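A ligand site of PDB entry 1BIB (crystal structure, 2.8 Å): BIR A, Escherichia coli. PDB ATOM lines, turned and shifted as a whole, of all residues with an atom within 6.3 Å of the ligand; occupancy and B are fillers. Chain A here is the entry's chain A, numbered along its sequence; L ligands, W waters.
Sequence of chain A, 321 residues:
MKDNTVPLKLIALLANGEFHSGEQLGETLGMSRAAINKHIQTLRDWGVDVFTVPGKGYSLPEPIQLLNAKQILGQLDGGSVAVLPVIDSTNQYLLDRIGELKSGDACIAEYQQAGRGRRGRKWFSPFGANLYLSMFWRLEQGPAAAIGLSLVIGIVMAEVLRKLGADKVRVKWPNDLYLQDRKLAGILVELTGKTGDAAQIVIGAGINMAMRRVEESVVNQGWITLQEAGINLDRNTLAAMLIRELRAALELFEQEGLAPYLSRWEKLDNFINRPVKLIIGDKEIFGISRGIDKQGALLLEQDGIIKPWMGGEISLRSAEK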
ATOM      1  N   ASP A  88      20.410  32.856   0.060  1.00  0.00           N
ATOM      2  CA  ASP A  88      21.403  32.194  -0.778  1.00  0.00           C
ATOM      3  C   ASP A  88      20.573  31.348  -1.782  1.00  0.00           C
ATOM      4  O   ASP A  88      20.327  31.745  -2.942  1.00  0.00           O
ATOM      5  CB  ASP A  88      22.277  31.317   0.168  1.00  0.00           C
ATOM      6  CG  ASP A  88      21.384  30.555   1.151  1.00  0.00           C
ATOM      7  OD1 ASP A  88      20.130  30.734   0.948  1.00  0.00           O
ATOM      8  OD2 ASP A  88      21.822  29.731   1.983  1.00  0.00           O
ATOM      9  N   SER A  89      20.019  30.240  -1.281  1.00  0.00           N
ATOM     10  CA  SER A  89      19.160  29.386  -2.030  1.00  0.00           C
ATOM     11  C   SER A  89      18.147  28.715  -1.092  1.00  0.00           C
ATOM     12  O   SER A  89      18.506  28.255   0.024  1.00  0.00           O
ATOM     13  CB  SER A  89      20.028  28.365  -2.698  1.00  0.00           C
ATOM     14  OG  SER A  89      19.610  27.107  -2.246  1.00  0.00           O
ATOM     15  N   THR A  90      16.875  28.638  -1.560  1.00  0.00           N
ATOM     16  CA  THR A  90      15.734  28.015  -0.827  1.00  0.00           C
ATOM     17  C   THR A  90      15.994  26.558  -0.602  1.00  0.00           C
ATOM     18  O   THR A  90      15.787  26.063   0.513  1.00  0.00           O
ATOM     19  CB  THR A  90      14.349  28.191  -1.494  1.00  0.00           C
ATOM     20  OG1 THR A  90      14.289  27.520  -2.743  1.00  0.00           O
ATOM     21  CG2 THR A  90      14.067  29.680  -1.743  1.00  0.00           C
ATOM     22  N   ASN A  91      16.544  25.897  -1.640  1.00  0.00           N
ATOM     23  CA  ASN A  91      16.866  24.483  -1.483  1.00  0.00           C
ATOM     24  C   ASN A  91      17.986  24.256  -0.451  1.00  0.00           C
ATOM     25  O   ASN A  91      17.913  23.487   0.512  1.00  0.00           O
ATOM     26  CB  ASN A  91      17.172  23.817  -2.816  1.00  0.00           C
ATOM     27  CG  ASN A  91      15.963  23.338  -3.598  1.00  0.00           C
ATOM     28  OD1 ASN A  91      14.815  23.655  -3.293  1.00  0.00           O
ATOM     29  ND2 ASN A  91      16.224  22.624  -4.685  1.00  0.00           N
ATOM     30  N   GLN A  92      19.054  24.977  -0.609  1.00  0.00           N
ATOM     31  CA  GLN A  92      20.137  24.882   0.328  1.00  0.00           C
ATOM     32  C   GLN A  92      19.638  25.099   1.748  1.00  0.00           C
ATOM     33  O   GLN A  92      19.867  24.329   2.693  1.00  0.00           O
ATOM     34  CB  GLN A  92      21.104  26.016   0.000  1.00  0.00           C
ATOM     35  CG  GLN A  92      22.552  25.653   0.368  1.00  0.00           C
ATOM     36  CD  GLN A  92      22.890  24.223   0.040  1.00  0.00           C
ATOM     37  OE1 GLN A  92      23.195  23.898  -1.117  1.00  0.00           O
ATOM     38  NE2 GLN A  92      22.860  23.365   1.074  1.00  0.00           N
ATOM     39  N   GLN A 112      17.371  35.221  -4.657  1.00  0.00           N
ATOM     40  CA  GLN A 112      18.340  34.166  -4.322  1.00  0.00           C
ATOM     41  C   GLN A 112      19.710  34.584  -4.757  1.00  0.00           C
ATOM     42  O   GLN A 112      19.978  34.876  -5.925  1.00  0.00           O
ATOM     43  CB  GLN A 112      18.032  32.767  -4.913  1.00  0.00           C
ATOM     44  CG  GLN A 112      17.115  31.910  -4.013  1.00  0.00           C
ATOM     45  CD  GLN A 112      16.952  30.482  -4.461  1.00  0.00           C
ATOM     46  OE1 GLN A 112      16.881  29.560  -3.652  1.00  0.00           O
ATOM     47  NE2 GLN A 112      16.868  30.287  -5.767  1.00  0.00           N
ATOM     48  N   ALA A 114      22.324  32.748  -4.573  1.00  0.00           N
ATOM     49  CA  ALA A 114      23.125  31.626  -4.985  1.00  0.00           C
ATOM     50  C   ALA A 114      22.190  30.478  -5.294  1.00  0.00           C
ATOM     51  O   ALA A 114      22.168  29.470  -4.576  1.00  0.00           O
ATOM     52  CB  ALA A 114      24.064  31.274  -3.853  1.00  0.00           C
ATOM     53  N   GLY A 115      21.405  30.650  -6.356  1.00  0.00           N
ATOM     54  CA  GLY A 115      20.483  29.611  -6.712  1.00  0.00           C
ATOM     55  C   GLY A 115      21.153  28.347  -7.283  1.00  0.00           C
ATOM     56  O   GLY A 115      22.053  28.442  -8.115  1.00  0.00           O
ATOM     57  N   ARG A 116      20.687  27.156  -6.831  1.00  0.00           N
ATOM     58  CA  ARG A 116      21.151  25.858  -7.305  1.00  0.00           C
ATOM     59  C   ARG A 116      20.375  25.531  -8.563  1.00  0.00           C
ATOM     60  O   ARG A 116      19.345  26.155  -8.790  1.00  0.00           O
ATOM     61  CB  ARG A 116      20.820  24.808  -6.267  1.00  0.00           C
ATOM     62  CG  ARG A 116      21.366  25.187  -4.905  1.00  0.00           C
ATOM     63  CD  ARG A 116      20.852  24.295  -3.782  1.00  0.00           C
ATOM     64  NE  ARG A 116      21.579  23.066  -3.490  1.00  0.00           N
ATOM     65  CZ  ARG A 116      22.441  22.431  -4.280  1.00  0.00           C
ATOM     66  NH1 ARG A 116      22.773  22.866  -5.495  1.00  0.00           N
ATOM     67  NH2 ARG A 116      23.026  21.304  -3.848  1.00  0.00           N
ATOM     68  N   GLY A 117      20.829  24.599  -9.411  1.00  0.00           N
ATOM     69  CA  GLY A 117      20.033  24.177 -10.568  1.00  0.00           C
ATOM     70  C   GLY A 117      20.085  24.825 -11.953  1.00  0.00           C
ATOM     71  O   GLY A 117      19.238  24.497 -12.795  1.00  0.00           O
ATOM     72  N   ARG A 118      21.086  25.669 -12.193  1.00  0.00           N
ATOM     73  CA  ARG A 118      21.378  26.375 -13.448  1.00  0.00           C
ATOM     74  C   ARG A 118      21.342  27.865 -13.174  1.00  0.00           C
ATOM     75  O   ARG A 118      22.196  28.617 -13.647  1.00  0.00           O
ATOM     76  CB  ARG A 118      20.570  26.021 -14.704  1.00  0.00           C
ATOM     77  CG  ARG A 118      20.884  24.649 -15.262  1.00  0.00           C
ATOM     78  CD  ARG A 118      19.813  24.079 -16.187  1.00  0.00           C
ATOM     79  NE  ARG A 118      20.428  23.282 -17.243  1.00  0.00           N
ATOM     80  CZ  ARG A 118      19.817  22.528 -18.188  1.00  0.00           C
ATOM     81  NH1 ARG A 118      18.473  22.403 -18.266  1.00  0.00           N
ATOM     82  NH2 ARG A 118      20.597  21.865 -19.048  1.00  0.00           N
ATOM     83  N   LEU A 131       9.539  34.125  -7.803  1.00  0.00           N
ATOM     84  CA  LEU A 131       9.051  33.535  -6.565  1.00  0.00           C
ATOM     85  C   LEU A 131       9.721  32.215  -6.347  1.00  0.00           C
ATOM     86  O   LEU A 131       9.739  31.383  -7.225  1.00  0.00           O
ATOM     87  CB  LEU A 131       7.525  33.393  -6.516  1.00  0.00           C
ATOM     88  CG  LEU A 131       7.020  32.708  -5.258  1.00  0.00           C
ATOM     89  CD1 LEU A 131       7.341  33.572  -4.063  1.00  0.00           C
ATOM     90  CD2 LEU A 131       5.515  32.522  -5.306  1.00  0.00           C
ATOM     91  N   TYR A 132      10.283  32.053  -5.171  1.00  0.00           N
ATOM     92  CA  TYR A 132      11.000  30.849  -4.886  1.00  0.00           C
ATOM     93  C   TYR A 132      10.375  30.050  -3.785  1.00  0.00           C
ATOM     94  O   TYR A 132      10.109  30.530  -2.688  1.00  0.00           O
ATOM     95  CB  TYR A 132      12.445  31.155  -4.529  1.00  0.00           C
ATOM     96  CG  TYR A 132      13.137  31.894  -5.629  1.00  0.00           C
ATOM     97  CD1 TYR A 132      13.438  31.227  -6.823  1.00  0.00           C
ATOM     98  CD2 TYR A 132      13.534  33.225  -5.471  1.00  0.00           C
ATOM     99  CE1 TYR A 132      14.077  31.902  -7.856  1.00  0.00           C
ATOM    100  CE2 TYR A 132      14.159  33.909  -6.508  1.00  0.00           C
ATOM    101  CZ  TYR A 132      14.419  33.235  -7.699  1.00  0.00           C
ATOM    102  OH  TYR A 132      15.063  33.868  -8.722  1.00  0.00           O
ATOM    103  N   LEU A 133      10.134  28.803  -4.073  1.00  0.00           N
ATOM    104  CA  LEU A 133       9.519  28.016  -3.083  1.00  0.00           C
ATOM    105  C   LEU A 133      10.206  26.691  -2.987  1.00  0.00           C
ATOM    106  O   LEU A 133      10.516  26.095  -4.028  1.00  0.00           O
ATOM    107  CB  LEU A 133       8.044  27.852  -3.529  1.00  0.00           C
ATOM    108  CG  LEU A 133       7.247  27.188  -2.417  1.00  0.00           C
ATOM    109  CD1 LEU A 133       5.802  27.641  -2.447  1.00  0.00           C
ATOM    110  CD2 LEU A 133       7.348  25.680  -2.539  1.00  0.00           C
ATOM    111  N   SER A 134      10.415  26.219  -1.770  1.00  0.00           N
ATOM    112  CA  SER A 134      11.017  24.907  -1.571  1.00  0.00           C
ATOM    113  C   SER A 134      10.353  24.178  -0.448  1.00  0.00           C
ATOM    114  O   SER A 134      10.044  24.747   0.578  1.00  0.00           O
ATOM    115  CB  SER A 134      12.518  24.862  -1.314  1.00  0.00           C
ATOM    116  OG  SER A 134      13.181  25.349  -2.431  1.00  0.00           O
ATOM    117  N   ASN A 175       9.241  18.759 -16.047  1.00  0.00           N
ATOM    118  CA  ASN A 175       9.476  19.687 -14.951  1.00  0.00           C
ATOM    119  C   ASN A 175       9.398  21.201 -15.165  1.00  0.00           C
ATOM    120  O   ASN A 175      10.020  21.917 -14.393  1.00  0.00           O
ATOM    121  CB  ASN A 175      10.884  19.385 -14.427  1.00  0.00           C
ATOM    122  CG  ASN A 175      11.901  19.648 -15.510  1.00  0.00           C
ATOM    123  OD1 ASN A 175      11.563  19.870 -16.692  1.00  0.00           O
ATOM    124  ND2 ASN A 175      13.151  19.653 -15.102  1.00  0.00           N
ATOM    125  N   ASP A 176       8.680  21.735 -16.120  1.00  0.00           N
ATOM    126  CA  ASP A 176       8.589  23.183 -16.195  1.00  0.00           C
ATOM    127  C   ASP A 176       7.179  23.541 -16.410  1.00  0.00           C
ATOM    128  O   ASP A 176       6.413  22.719 -16.869  1.00  0.00           O
ATOM    129  CB  ASP A 176       9.283  23.767 -17.426  1.00  0.00           C
ATOM    130  CG  ASP A 176      10.723  23.430 -17.366  1.00  0.00           C
ATOM    131  OD1 ASP A 176      11.117  23.146 -16.147  1.00  0.00           O
ATOM    132  OD2 ASP A 176      11.462  23.432 -18.337  1.00  0.00           O
ATOM    133  N   LYS A 183       8.969  29.335 -21.184  1.00  0.00           N
ATOM    134  CA  LYS A 183       9.164  28.830 -19.845  1.00  0.00           C
ATOM    135  C   LYS A 183       8.720  29.817 -18.738  1.00  0.00           C
ATOM    136  O   LYS A 183       9.036  30.987 -18.736  1.00  0.00           O
ATOM    137  CB  LYS A 183      10.493  28.136 -19.686  1.00  0.00           C
ATOM    138  CG  LYS A 183      10.823  27.908 -18.240  1.00  0.00           C
ATOM    139  CD  LYS A 183      12.048  27.063 -18.030  1.00  0.00           C
ATOM    140  CE  LYS A 183      12.052  26.488 -16.626  1.00  0.00           C
ATOM    141  NZ  LYS A 183      13.394  26.380 -16.076  1.00  0.00           N
ATOM    142  N   ALA A 185       8.099  28.527 -15.205  1.00  0.00           N
ATOM    143  CA  ALA A 185       8.589  28.068 -13.903  1.00  0.00           C
ATOM    144  C   ALA A 185       9.430  26.845 -14.066  1.00  0.00           C
ATOM    145  O   ALA A 185       9.377  26.213 -15.111  1.00  0.00           O
ATOM    146  CB  ALA A 185       7.536  27.816 -12.842  1.00  0.00           C
ATOM    147  N   GLY A 186      10.168  26.520 -13.011  1.00  0.00           N
ATOM    148  CA  GLY A 186      11.019  25.372 -13.088  1.00  0.00           C
ATOM    149  C   GLY A 186      11.133  24.641 -11.801  1.00  0.00           C
ATOM    150  O   GLY A 186      11.458  25.209 -10.770  1.00  0.00           O
ATOM    151  N   ILE A 187      10.822  23.356 -11.855  1.00  0.00           N
ATOM    152  CA  ILE A 187      10.917  22.548 -10.677  1.00  0.00           C
ATOM    153  C   ILE A 187      12.340  22.006 -10.600  1.00  0.00           C
ATOM    154  O   ILE A 187      13.030  21.972 -11.606  1.00  0.00           O
ATOM    155  CB  ILE A 187       9.856  21.439 -10.654  1.00  0.00           C
ATOM    156  CG1 ILE A 187       8.445  21.975 -10.713  1.00  0.00           C
ATOM    157  CG2 ILE A 187       9.955  20.612  -9.383  1.00  0.00           C
ATOM    158  CD1 ILE A 187       7.830  22.019 -12.096  1.00  0.00           C
ATOM    159  N   LEU A 188      12.782  21.656  -9.403  1.00  0.00           N
ATOM    160  CA  LEU A 188      14.057  21.035  -9.159  1.00  0.00           C
ATOM    161  C   LEU A 188      13.946  20.039  -7.979  1.00  0.00           C
ATOM    162  O   LEU A 188      13.644  20.386  -6.834  1.00  0.00           O
ATOM    163  CB  LEU A 188      15.233  21.992  -8.962  1.00  0.00           C
ATOM    164  CG  LEU A 188      16.435  21.220  -8.384  1.00  0.00           C
ATOM    165  CD1 LEU A 188      17.124  20.484  -9.488  1.00  0.00           C
ATOM    166  CD2 LEU A 188      17.470  22.101  -7.720  1.00  0.00           C
ATOM    167  N   GLU A 190      15.694  17.119  -5.458  1.00  0.00           N
ATOM    168  CA  GLU A 190      16.944  16.667  -4.920  1.00  0.00           C
ATOM    169  C   GLU A 190      16.727  15.579  -3.924  1.00  0.00           C
ATOM    170  O   GLU A 190      16.105  15.851  -2.914  1.00  0.00           O
ATOM    171  CB  GLU A 190      17.615  17.806  -4.131  1.00  0.00           C
ATOM    172  CG  GLU A 190      17.868  19.085  -4.948  1.00  0.00           C
ATOM    173  CD  GLU A 190      19.080  19.804  -4.427  1.00  0.00           C
ATOM    174  OE1 GLU A 190      19.985  19.192  -3.883  1.00  0.00           O
ATOM    175  OE2 GLU A 190      19.046  21.116  -4.587  1.00  0.00           O
ATOM    176  N   ILE A 203      12.123  19.830  -2.555  1.00  0.00           N
ATOM    177  CA  ILE A 203      11.519  20.297  -3.787  1.00  0.00           C
ATOM    178  C   ILE A 203      11.744  21.762  -3.860  1.00  0.00           C
ATOM    179  O   ILE A 203      11.743  22.393  -2.807  1.00  0.00           O
ATOM    180  CB  ILE A 203      10.023  19.978  -3.817  1.00  0.00           C
ATOM    181  CG1 ILE A 203       9.834  18.525  -3.420  1.00  0.00           C
ATOM    182  CG2 ILE A 203       9.507  20.183  -5.232  1.00  0.00           C
ATOM    183  CD1 ILE A 203       8.614  18.305  -2.543  1.00  0.00           C
ATOM    184  N   GLY A 204      11.932  22.289  -5.058  1.00  0.00           N
ATOM    185  CA  GLY A 204      12.183  23.691  -5.171  1.00  0.00           C
ATOM    186  C   GLY A 204      11.704  24.231  -6.477  1.00  0.00           C
ATOM    187  O   GLY A 204      11.998  23.730  -7.521  1.00  0.00           O
ATOM    188  N   ALA A 205      11.000  25.309  -6.430  1.00  0.00           N
ATOM    189  CA  ALA A 205      10.522  25.812  -7.675  1.00  0.00           C
ATOM    190  C   ALA A 205      10.698  27.310  -7.653  1.00  0.00           C
ATOM    191  O   ALA A 205      10.687  27.904  -6.549  1.00  0.00           O
ATOM    192  CB  ALA A 205       9.041  25.461  -7.784  1.00  0.00           C
ATOM    193  N   GLY A 206      10.803  27.859  -8.882  1.00  0.00           N
ATOM    194  CA  GLY A 206      10.962  29.292  -9.147  1.00  0.00           C
ATOM    195  C   GLY A 206       9.954  29.757 -10.205  1.00  0.00           C
ATOM    196  O   GLY A 206       9.786  29.176 -11.270  1.00  0.00           O
HETATM  197  C1  LIG L   1      15.019  26.903 -12.581  1.00  0.00           C
HETATM  198  O1  LIG L   1      16.027  27.450 -11.981  1.00  0.00           O
HETATM  199  O2  LIG L   1      14.457  27.495 -13.404  1.00  0.00           O
HETATM  200  C2  LIG L   1      14.740  25.419 -12.554  1.00  0.00           C
HETATM  201  C3  LIG L   1      15.245  24.909 -11.641  1.00  0.00           C
HETATM  202  C4  LIG L   1      14.447  25.659 -10.372  1.00  0.00           C
HETATM  203  C5  LIG L   1      15.526  25.944  -9.305  1.00  0.00           C
HETATM  204  C6  LIG L   1      14.799  26.110  -7.874  1.00  0.00           C
HETATM  205  S1  LIG L   1      14.507  27.808  -7.544  1.00  0.00           S
HETATM  206  C7  LIG L   1      14.150  27.428  -5.751  1.00  0.00           C
HETATM  207  C8  LIG L   1      15.150  26.289  -5.363  1.00  0.00           C
HETATM  208  N1  LIG L   1      16.285  26.949  -4.758  1.00  0.00           N
HETATM  209  C9  LIG L   1      17.422  26.762  -5.521  1.00  0.00           C
HETATM  210  O3  LIG L   1      18.543  27.089  -5.074  1.00  0.00           O
HETATM  211  N2  LIG L   1      17.042  26.211  -6.695  1.00  0.00           N
HETATM  212  C10 LIG L   1      15.772  25.749  -6.705  1.00  0.00           C
HETATM  213  O   HOH W   1      15.164  22.413 -14.068  1.00  0.00           O
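OG of Ser 89 lies within hydrogen-bond range of N of Gln 92 (2.7 Å).
The backbone carbonyl oxygen (O) of Gly 204 is in hydrogen-bond range of the backbone NH (N) of Leu 188 (2.9 Å).
The backbone NH (N) of Gly 186 sits at hydrogen-bond distance from the backbone carbonyl oxygen (O) of Gly 206, 3.2 Å away.
The backbone NH (N) of Ala 205 lies within hydrogen-bond range of the backbone carbonyl oxygen (O) of Leu 133, at 2.6 Å.
The side-chain carboxylate (OE2) of Glu 190 sits at hydrogen-bond distance from the side-chain amide nitrogen (ND2) of Asn 91, at 3.2 Å.
The side-chain amide oxygen of Gln 112 sits close to the side-chain hydroxyl of Thr 90, 3.4 Å away.
NZ of Lys 183 is in salt-bridge range of OD1 of Asp 176 (3.96 Å).
OG of Ser 134 lies close to O of Ile 203.
The side-chain amide oxygen (OE1) of Gln 112 is in hydrogen-bond range of a nitrogen (N1) of the ligand (2.9 Å).
The side-chain hydroxyl (OG) of Ser 89 is in hydrogen-bond range of an oxygen (O3) of the ligand.
The backbone NH (N) of Arg 116 lies within hydrogen-bond range of an oxygen (O3) of the ligand, at 2.8 Å.
An oxygen (O2) of the ligand lies within salt-bridge range of the side-chain amino group (NZ) of Lys 183.
O of Arg 116 sits at hydrogen-bond distance from N2 of the ligand, at 3.1 Å.
N1 of the ligand sits at hydrogen-bond distance from OG1 of Thr 90 (2.9 Å).
The backbone NH (N) of Asn 91 sits close to a nitrogen (N1) of the ligand, 3.3 Å away.
Merely in contact with the ligand: Gly 186, Gly 115, Ala 205, Tyr 132, Ser 134, Ile 187, Gly 204, Gly 206 and Leu 188.
15 residues have an atom within 4 Å of the ligand: Ser 89, Thr 90, Asn 91, Gln 112, Gly 115, Arg 116, Tyr 132, Ser 134, Lys 183, Gly 186, Ile 187, Leu 188, Gly 204, Ala 205 and Gly 206.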
